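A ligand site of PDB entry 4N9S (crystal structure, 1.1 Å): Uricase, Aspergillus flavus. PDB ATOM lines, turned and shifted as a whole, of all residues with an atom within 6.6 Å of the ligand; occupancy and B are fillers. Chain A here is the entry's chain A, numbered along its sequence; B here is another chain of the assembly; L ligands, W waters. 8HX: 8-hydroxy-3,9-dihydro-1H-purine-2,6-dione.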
ATOM      1  N   SER A 158      10.092  30.566 -20.195  1.00  0.00           N
ATOM      2  CA  SER A 158      10.859  29.606 -19.437  1.00  0.00           C
ATOM      3  C   SER A 158      10.356  29.699 -18.003  1.00  0.00           C
ATOM      4  O   SER A 158      10.110  30.805 -17.501  1.00  0.00           O
ATOM      5  CB  SER A 158      12.345  29.912 -19.537  1.00  0.00           C
ATOM      6  OG  SER A 158      13.108  29.132 -18.645  1.00  0.00           O
ATOM      7  N   GLN A 159      10.193  28.541 -17.369  1.00  0.00           N
ATOM      8  CA  GLN A 159       9.686  28.410 -16.008  1.00  0.00           C
ATOM      9  C   GLN A 159      10.583  27.475 -15.224  1.00  0.00           C
ATOM     10  O   GLN A 159      11.280  26.628 -15.801  1.00  0.00           O
ATOM     11  CB  GLN A 159       8.242  27.867 -16.018  1.00  0.00           C
ATOM     12  CG  GLN A 159       7.359  28.584 -16.998  1.00  0.00           C
ATOM     13  CD  GLN A 159       5.907  28.231 -16.882  1.00  0.00           C
ATOM     14  OE1 GLN A 159       5.412  27.947 -15.793  1.00  0.00           O
ATOM     15  NE2 GLN A 159       5.203  28.244 -17.996  1.00  0.00           N
ATOM     16  N   PHE A 160      10.526  27.566 -13.899  1.00  0.00           N
ATOM     17  CA  PHE A 160      11.155  26.565 -13.059  1.00  0.00           C
ATOM     18  C   PHE A 160      10.523  26.610 -11.671  1.00  0.00           C
ATOM     19  O   PHE A 160      10.833  27.465 -10.844  1.00  0.00           O
ATOM     20  CB  PHE A 160      12.687  26.732 -12.993  1.00  0.00           C
ATOM     21  CG  PHE A 160      13.373  25.540 -12.375  1.00  0.00           C
ATOM     22  CD1 PHE A 160      13.262  24.290 -12.972  1.00  0.00           C
ATOM     23  CD2 PHE A 160      14.096  25.663 -11.202  1.00  0.00           C
ATOM     24  CE1 PHE A 160      13.873  23.192 -12.421  1.00  0.00           C
ATOM     25  CE2 PHE A 160      14.712  24.554 -10.643  1.00  0.00           C
ATOM     26  CZ  PHE A 160      14.595  23.314 -11.263  1.00  0.00           C
ATOM     27  N   PHE A 163      10.453  22.135  -7.838  1.00  0.00           N
ATOM     28  CA  PHE A 163      11.661  21.438  -7.467  1.00  0.00           C
ATOM     29  C   PHE A 163      11.713  21.161  -5.961  1.00  0.00           C
ATOM     30  O   PHE A 163      10.952  21.734  -5.179  1.00  0.00           O
ATOM     31  CB  PHE A 163      12.892  22.230  -7.943  1.00  0.00           C
ATOM     32  CG  PHE A 163      12.897  23.672  -7.527  1.00  0.00           C
ATOM     33  CD1 PHE A 163      12.355  24.644  -8.362  1.00  0.00           C
ATOM     34  CD2 PHE A 163      13.431  24.069  -6.317  1.00  0.00           C
ATOM     35  CE1 PHE A 163      12.354  25.978  -8.014  1.00  0.00           C
ATOM     36  CE2 PHE A 163      13.444  25.401  -5.956  1.00  0.00           C
ATOM     37  CZ  PHE A 163      12.898  26.352  -6.803  1.00  0.00           C
ATOM     38  N   LEU A 171      16.244  29.133  -3.549  1.00  0.00           N
ATOM     39  CA  LEU A 171      15.726  29.560  -4.844  1.00  0.00           C
ATOM     40  C   LEU A 171      14.209  29.694  -4.851  1.00  0.00           C
ATOM     41  O   LEU A 171      13.499  28.783  -4.464  1.00  0.00           O
ATOM     42  CB  LEU A 171      16.133  28.545  -5.916  1.00  0.00           C
ATOM     43  CG  LEU A 171      15.719  28.849  -7.370  1.00  0.00           C
ATOM     44  CD1 LEU A 171      16.416  30.099  -7.912  1.00  0.00           C
ATOM     45  CD2 LEU A 171      16.012  27.663  -8.258  1.00  0.00           C
ATOM     46  N   ARG A 177      10.988  33.370 -16.510  1.00  0.00           N
ATOM     47  CA  ARG A 177      12.405  33.724 -16.383  1.00  0.00           C
ATOM     48  C   ARG A 177      13.045  33.770 -17.765  1.00  0.00           C
ATOM     49  O   ARG A 177      12.465  33.303 -18.746  1.00  0.00           O
ATOM     50  CB  ARG A 177      13.155  32.731 -15.479  1.00  0.00           C
ATOM     51  CG  ARG A 177      13.250  31.333 -16.054  1.00  0.00           C
ATOM     52  CD  ARG A 177      14.034  30.369 -15.197  1.00  0.00           C
ATOM     53  NE  ARG A 177      14.159  29.086 -15.890  1.00  0.00           N
ATOM     54  CZ  ARG A 177      14.907  28.067 -15.475  1.00  0.00           C
ATOM     55  NH1 ARG A 177      15.525  28.111 -14.304  1.00  0.00           N
ATOM     56  NH2 ARG A 177      15.035  26.992 -16.243  1.00  0.00           N
ATOM     57  N   LEU A 179      15.945  32.340 -20.225  1.00  0.00           N
ATOM     58  CA  LEU A 179      16.746  31.137 -20.407  1.00  0.00           C
ATOM     59  C   LEU A 179      17.756  31.391 -21.522  1.00  0.00           C
ATOM     60  O   LEU A 179      17.378  31.740 -22.640  1.00  0.00           O
ATOM     61  CB  LEU A 179      15.863  29.935 -20.761  1.00  0.00           C
ATOM     62  CG  LEU A 179      16.606  28.629 -21.074  1.00  0.00           C
ATOM     63  CD1 LEU A 179      17.468  28.171 -19.916  1.00  0.00           C
ATOM     64  CD2 LEU A 179      15.625  27.548 -21.482  1.00  0.00           C
ATOM     65  N   SER A 225       9.134  26.309 -21.484  1.00  0.00           N
ATOM     66  CA  SER A 225      10.008  25.332 -20.873  1.00  0.00           C
ATOM     67  C   SER A 225       9.740  25.117 -19.383  1.00  0.00           C
ATOM     68  O   SER A 225       9.737  26.071 -18.604  1.00  0.00           O
ATOM     69  CB  SER A 225      11.450  25.780 -21.096  1.00  0.00           C
ATOM     70  OG  SER A 225      12.358  24.990 -20.375  1.00  0.00           O
ATOM     71  N   ALA A 226       9.545  23.860 -18.995  1.00  0.00           N
ATOM     72  CA  ALA A 226       9.391  23.497 -17.591  1.00  0.00           C
ATOM     73  C   ALA A 226      10.721  23.417 -16.846  1.00  0.00           C
ATOM     74  O   ALA A 226      10.747  23.470 -15.615  1.00  0.00           O
ATOM     75  CB  ALA A 226       8.666  22.160 -17.486  1.00  0.00           C
ATOM     76  N   SER A 227      11.810  23.244 -17.608  1.00  0.00           N
ATOM     77  CA  SER A 227      13.165  23.092 -17.108  1.00  0.00           C
ATOM     78  C   SER A 227      14.062  22.910 -18.314  1.00  0.00           C
ATOM     79  O   SER A 227      13.603  22.540 -19.394  1.00  0.00           O
ATOM     80  CB  SER A 227      13.338  21.872 -16.210  1.00  0.00           C
ATOM     81  OG  SER A 227      13.135  20.683 -16.936  1.00  0.00           O
ATOM     82  N   VAL A 228      15.363  23.101 -18.131  1.00  0.00           N
ATOM     83  CA  VAL A 228      16.302  22.768 -19.198  1.00  0.00           C
ATOM     84  C   VAL A 228      16.207  21.272 -19.541  1.00  0.00           C
ATOM     85  O   VAL A 228      16.196  20.901 -20.717  1.00  0.00           O
ATOM     86  CB  VAL A 228      17.721  23.180 -18.799  1.00  0.00           C
ATOM     87  CG1 VAL A 228      18.714  22.771 -19.877  1.00  0.00           C
ATOM     88  CG2 VAL A 228      17.813  24.685 -18.585  1.00  0.00           C
ATOM     89  N   GLN A 229      16.084  20.443 -18.504  1.00  0.00           N
ATOM     90  CA  GLN A 229      15.957  18.995 -18.644  1.00  0.00           C
ATOM     91  C   GLN A 229      14.815  18.639 -19.610  1.00  0.00           C
ATOM     92  O   GLN A 229      14.989  17.816 -20.537  1.00  0.00           O
ATOM     93  CB  GLN A 229      15.668  18.370 -17.281  1.00  0.00           C
ATOM     94  CG  GLN A 229      16.841  18.331 -16.276  1.00  0.00           C
ATOM     95  CD  GLN A 229      17.050  19.591 -15.442  1.00  0.00           C
ATOM     96  OE1 GLN A 229      16.625  20.708 -15.792  1.00  0.00           O
ATOM     97  NE2 GLN A 229      17.738  19.417 -14.335  1.00  0.00           N
ATOM     98  N   ASN A 255      23.061  26.516 -18.004  1.00  0.00           N
ATOM     99  CA  ASN A 255      22.014  27.496 -17.739  1.00  0.00           C
ATOM    100  C   ASN A 255      22.737  28.781 -17.334  1.00  0.00           C
ATOM    101  O   ASN A 255      23.295  28.862 -16.241  1.00  0.00           O
ATOM    102  CB  ASN A 255      21.093  26.972 -16.642  1.00  0.00           C
ATOM    103  CG  ASN A 255      19.793  27.767 -16.547  1.00  0.00           C
ATOM    104  OD1 ASN A 255      19.584  28.745 -17.266  1.00  0.00           O
ATOM    105  ND2 ASN A 255      18.908  27.337 -15.666  1.00  0.00           N
ATOM    106  N   HIS A 257      22.794  32.129 -16.188  1.00  0.00           N
ATOM    107  CA  HIS A 257      21.754  32.817 -15.415  1.00  0.00           C
ATOM    108  C   HIS A 257      21.765  34.318 -15.644  1.00  0.00           C
ATOM    109  O   HIS A 257      22.826  34.950 -15.727  1.00  0.00           O
ATOM    110  CB  HIS A 257      21.934  32.530 -13.915  1.00  0.00           C
ATOM    111  CG  HIS A 257      22.004  31.074 -13.560  1.00  0.00           C
ATOM    112  ND1 HIS A 257      20.961  30.194 -13.755  1.00  0.00           N
ATOM    113  CD2 HIS A 257      23.018  30.334 -13.033  1.00  0.00           C
ATOM    114  CE1 HIS A 257      21.329  28.981 -13.372  1.00  0.00           C
ATOM    115  NE2 HIS A 257      22.564  29.038 -12.919  1.00  0.00           N
ATOM    116  N   GLY A 287      24.342  26.596 -14.051  1.00  0.00           N
ATOM    117  CA  GLY A 287      23.824  25.236 -14.112  1.00  0.00           C
ATOM    118  C   GLY A 287      24.448  24.511 -15.300  1.00  0.00           C
ATOM    119  O   GLY A 287      24.808  25.134 -16.296  1.00  0.00           O
ATOM    120  N   ILE A 289      23.485  20.939 -17.408  1.00  0.00           N
ATOM    121  CA  ILE A 289      22.454  19.909 -17.519  1.00  0.00           C
ATOM    122  C   ILE A 289      22.821  19.016 -18.707  1.00  0.00           C
ATOM    123  O   ILE A 289      23.074  19.510 -19.801  1.00  0.00           O
ATOM    124  CB  ILE A 289      21.063  20.549 -17.747  1.00  0.00           C
ATOM    125  CG1 ILE A 289      20.801  21.772 -16.828  1.00  0.00           C
ATOM    126  CG2 ILE A 289      19.968  19.493 -17.647  1.00  0.00           C
ATOM    127  CD1 ILE A 289      20.929  21.577 -15.362  1.00  0.00           C
ATOM    128  N   TYR B   9      23.291  16.283 -13.822  1.00  0.00           N
ATOM    129  CA  TYR B   9      23.046  17.719 -13.846  1.00  0.00           C
ATOM    130  C   TYR B   9      23.559  18.316 -12.539  1.00  0.00           C
ATOM    131  O   TYR B   9      23.658  17.631 -11.513  1.00  0.00           O
ATOM    132  CB  TYR B   9      21.535  18.029 -14.039  1.00  0.00           C
ATOM    133  CG  TYR B   9      20.843  17.949 -12.708  1.00  0.00           C
ATOM    134  CD1 TYR B   9      20.574  16.719 -12.119  1.00  0.00           C
ATOM    135  CD2 TYR B   9      20.556  19.096 -11.995  1.00  0.00           C
ATOM    136  CE1 TYR B   9      20.057  16.654 -10.842  1.00  0.00           C
ATOM    137  CE2 TYR B   9      20.055  19.039 -10.719  1.00  0.00           C
ATOM    138  CZ  TYR B   9      19.801  17.813 -10.145  1.00  0.00           C
ATOM    139  OH  TYR B   9      19.305  17.743  -8.876  1.00  0.00           O
ATOM    140  N   GLY B  10      23.855  19.608 -12.545  1.00  0.00           N
ATOM    141  CA  GLY B  10      24.301  20.243 -11.323  1.00  0.00           C
ATOM    142  C   GLY B  10      24.809  21.638 -11.570  1.00  0.00           C
ATOM    143  O   GLY B  10      24.342  22.316 -12.484  1.00  0.00           O
ATOM    144  N   LYS B  11      25.722  22.087 -10.713  1.00  0.00           N
ATOM    145  CA  LYS B  11      26.256  23.447 -10.830  1.00  0.00           C
ATOM    146  C   LYS B  11      27.742  23.383 -11.132  1.00  0.00           C
ATOM    147  O   LYS B  11      28.487  22.679 -10.445  1.00  0.00           O
ATOM    148  CB  LYS B  11      26.001  24.280  -9.565  1.00  0.00           C
ATOM    149  CG  LYS B  11      26.193  25.773  -9.767  1.00  0.00           C
ATOM    150  CD  LYS B  11      25.074  26.418 -10.564  1.00  0.00           C
ATOM    151  CE  LYS B  11      24.084  27.146  -9.691  1.00  0.00           C
ATOM    152  NZ  LYS B  11      22.847  27.471 -10.455  1.00  0.00           N
ATOM    153  N   ASN B  52       9.745  18.096 -11.789  1.00  0.00           N
ATOM    154  CA  ASN B  52      10.814  18.765 -11.066  1.00  0.00           C
ATOM    155  C   ASN B  52      10.975  18.312  -9.629  1.00  0.00           C
ATOM    156  O   ASN B  52      11.932  18.701  -8.975  1.00  0.00           O
ATOM    157  CB  ASN B  52      10.689  20.289 -11.175  1.00  0.00           C
ATOM    158  CG  ASN B  52      10.983  20.786 -12.563  1.00  0.00           C
ATOM    159  OD1 ASN B  52      11.740  20.156 -13.304  1.00  0.00           O
ATOM    160  ND2 ASN B  52      10.391  21.907 -12.939  1.00  0.00           N
ATOM    161  N   ILE B  55      14.347  17.033  -8.701  1.00  0.00           N
ATOM    162  CA  ILE B  55      15.491  17.905  -8.881  1.00  0.00           C
ATOM    163  C   ILE B  55      15.843  18.622  -7.575  1.00  0.00           C
ATOM    164  O   ILE B  55      15.045  19.416  -7.045  1.00  0.00           O
ATOM    165  CB  ILE B  55      15.250  18.933 -10.014  1.00  0.00           C
ATOM    166  CG1 ILE B  55      15.071  18.213 -11.357  1.00  0.00           C
ATOM    167  CG2 ILE B  55      16.398  19.928 -10.091  1.00  0.00           C
ATOM    168  CD1 ILE B  55      16.253  17.301 -11.770  1.00  0.00           C
ATOM    169  N   VAL B  56      17.031  18.314  -7.066  1.00  0.00           N
ATOM    170  CA  VAL B  56      17.720  19.157  -6.103  1.00  0.00           C
ATOM    171  C   VAL B  56      18.238  20.337  -6.935  1.00  0.00           C
ATOM    172  O   VAL B  56      19.081  20.158  -7.819  1.00  0.00           O
ATOM    173  CB  VAL B  56      18.876  18.379  -5.410  1.00  0.00           C
ATOM    174  CG1 VAL B  56      19.638  19.285  -4.470  1.00  0.00           C
ATOM    175  CG2 VAL B  56      18.329  17.147  -4.656  1.00  0.00           C
ATOM    176  N   ALA B  57      17.708  21.543  -6.718  1.00  0.00           N
ATOM    177  CA  ALA B  57      18.011  22.653  -7.612  1.00  0.00           C
ATOM    178  C   ALA B  57      19.508  22.877  -7.677  1.00  0.00           C
ATOM    179  O   ALA B  57      20.212  22.792  -6.677  1.00  0.00           O
ATOM    180  CB  ALA B  57      17.305  23.914  -7.155  1.00  0.00           C
ATOM    181  N   THR B  58      19.994  23.236  -8.864  1.00  0.00           N
ATOM    182  CA  THR B  58      21.413  23.535  -8.981  1.00  0.00           C
ATOM    183  C   THR B  58      21.809  24.717  -8.080  1.00  0.00           C
ATOM    184  O   THR B  58      22.907  24.733  -7.530  1.00  0.00           O
ATOM    185  CB  THR B  58      21.843  23.786 -10.447  1.00  0.00           C
ATOM    186  OG1 THR B  58      21.353  25.074 -10.879  1.00  0.00           O
ATOM    187  CG2 THR B  58      21.356  22.685 -11.371  1.00  0.00           C
ATOM    188  N   ASP B  59      20.889  25.654  -7.854  1.00  0.00           N
ATOM    189  CA  ASP B  59      21.131  26.732  -6.908  1.00  0.00           C
ATOM    190  C   ASP B  59      21.344  26.193  -5.494  1.00  0.00           C
ATOM    191  O   ASP B  59      22.168  26.715  -4.738  1.00  0.00           O
ATOM    192  CB  ASP B  59      19.965  27.712  -6.928  1.00  0.00           C
ATOM    193  CG  ASP B  59      20.255  28.951  -6.126  1.00  0.00           C
ATOM    194  OD1 ASP B  59      20.929  29.855  -6.666  1.00  0.00           O
ATOM    195  OD2 ASP B  59      19.812  29.025  -4.950  1.00  0.00           O
ATOM    196  N   SER B  60      20.591  25.165  -5.138  1.00  0.00           N
ATOM    197  CA  SER B  60      20.758  24.511  -3.840  1.00  0.00           C
ATOM    198  C   SER B  60      22.063  23.743  -3.746  1.00  0.00           C
ATOM    199  O   SER B  60      22.677  23.694  -2.688  1.00  0.00           O
ATOM    200  CB  SER B  60      19.588  23.573  -3.554  1.00  0.00           C
ATOM    201  OG  SER B  60      18.376  24.277  -3.655  1.00  0.00           O
HETATM  202  N1  8HX L   1      17.014  23.141 -14.138  1.00  0.00           N
HETATM  203  C2  8HX L   1      16.596  24.392 -14.563  1.00  0.00           C
HETATM  204  O2  8HX L   1      16.061  24.440 -15.661  1.00  0.00           O
HETATM  205  N3  8HX L   1      16.756  25.508 -13.743  1.00  0.00           N
HETATM  206  C4  8HX L   1      17.338  25.298 -12.513  1.00  0.00           C
HETATM  207  C5  8HX L   1      17.748  24.041 -12.065  1.00  0.00           C
HETATM  208  C6  8HX L   1      17.594  22.923 -12.893  1.00  0.00           C
HETATM  209  O6  8HX L   1      17.937  21.769 -12.592  1.00  0.00           O
HETATM  210  N7  8HX L   1      18.195  24.183 -10.816  1.00  0.00           N
HETATM  211  C8  8HX L   1      18.138  25.504 -10.527  1.00  0.00           C
HETATM  212  O8  8HX L   1      18.561  26.054  -9.382  1.00  0.00           O
HETATM  213  N9  8HX L   1      17.611  26.165 -11.543  1.00  0.00           N
HETATM  214  O   HOH W   1      17.583  29.052 -11.831  1.00  0.00           O
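The guanidinium group (NH2) of Arg 177 sits at hydrogen-bond distance from an oxygen (O2) of the ligand (2.8 Å). The backbone NH of Asp 59 of chain B sits at hydrogen-bond distance from an oxygen (O8) of the ligand (2.8 Å). The backbone NH (N) of Thr 58 of chain B is in hydrogen-bond range of a nitrogen (N7) of the ligand, 2.8 Å away. A nitrogen (N7) of the ligand lies close to the side-chain hydroxyl (OG1) of Thr 58 of chain B (3.3 Å). N of Val 228 sits at hydrogen-bond distance from O2 of the ligand, at 2.9 Å. O6 of the ligand sits at hydrogen-bond distance from NE2 of Gln 229 (2.9 Å). ND2 of Asn 255 lies close to N3 of the ligand, at 3.4 Å.
The backbone carbonyl oxygen of Ser 158 lies within hydrogen-bond range of the backbone NH of Arg 177. OG1 of Thr 58 of chain B is in hydrogen-bond range of NZ of Lys 11 of chain B, at 2.9 Å. The side-chain hydroxyl (OG) of Ser 227 lies close to the backbone NH (N) of Gln 229, 3.3 Å away. NE2 of His 257 lies within hydrogen-bond range of O of Asn 255. N of Asn 255 lies within hydrogen-bond range of O of Gly 287 (2.8 Å). The backbone carbonyl oxygen (O) of Ser 227 sits at hydrogen-bond distance from the side-chain hydroxyl (OG) of Ser 225, at 2.9 Å. The backbone carbonyl oxygen (O) of Val 56 of chain B is in hydrogen-bond range of the side-chain hydroxyl (OH) of Tyr 9 of chain B, at 2.6 Å.
Merely in contact with the ligand: Phe 160, Leu 171, Ser 227, Tyr 9 of chain B, Ile 55 of chain B and Ala 57 of chain B. Hydrophobic or aromatic side chains that line the ligand: Phe 160, Leu 171, Val 228, Tyr 9 of chain B, Ile 55 of chain B and Ala 57 of chain B. Within 4 Å of the ligand: Phe 160, Leu 171, Arg 177, Ser 227, Val 228, Gln 229, Asn 255, Tyr 9 of chain B, Ile 55 of chain B, Ala 57 of chain B, Thr 58 of chain B and Asp 59 of chain B.
Water W1 lies within hydrogen-bond range of N9 of the ligand and NH1 of Arg 177.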
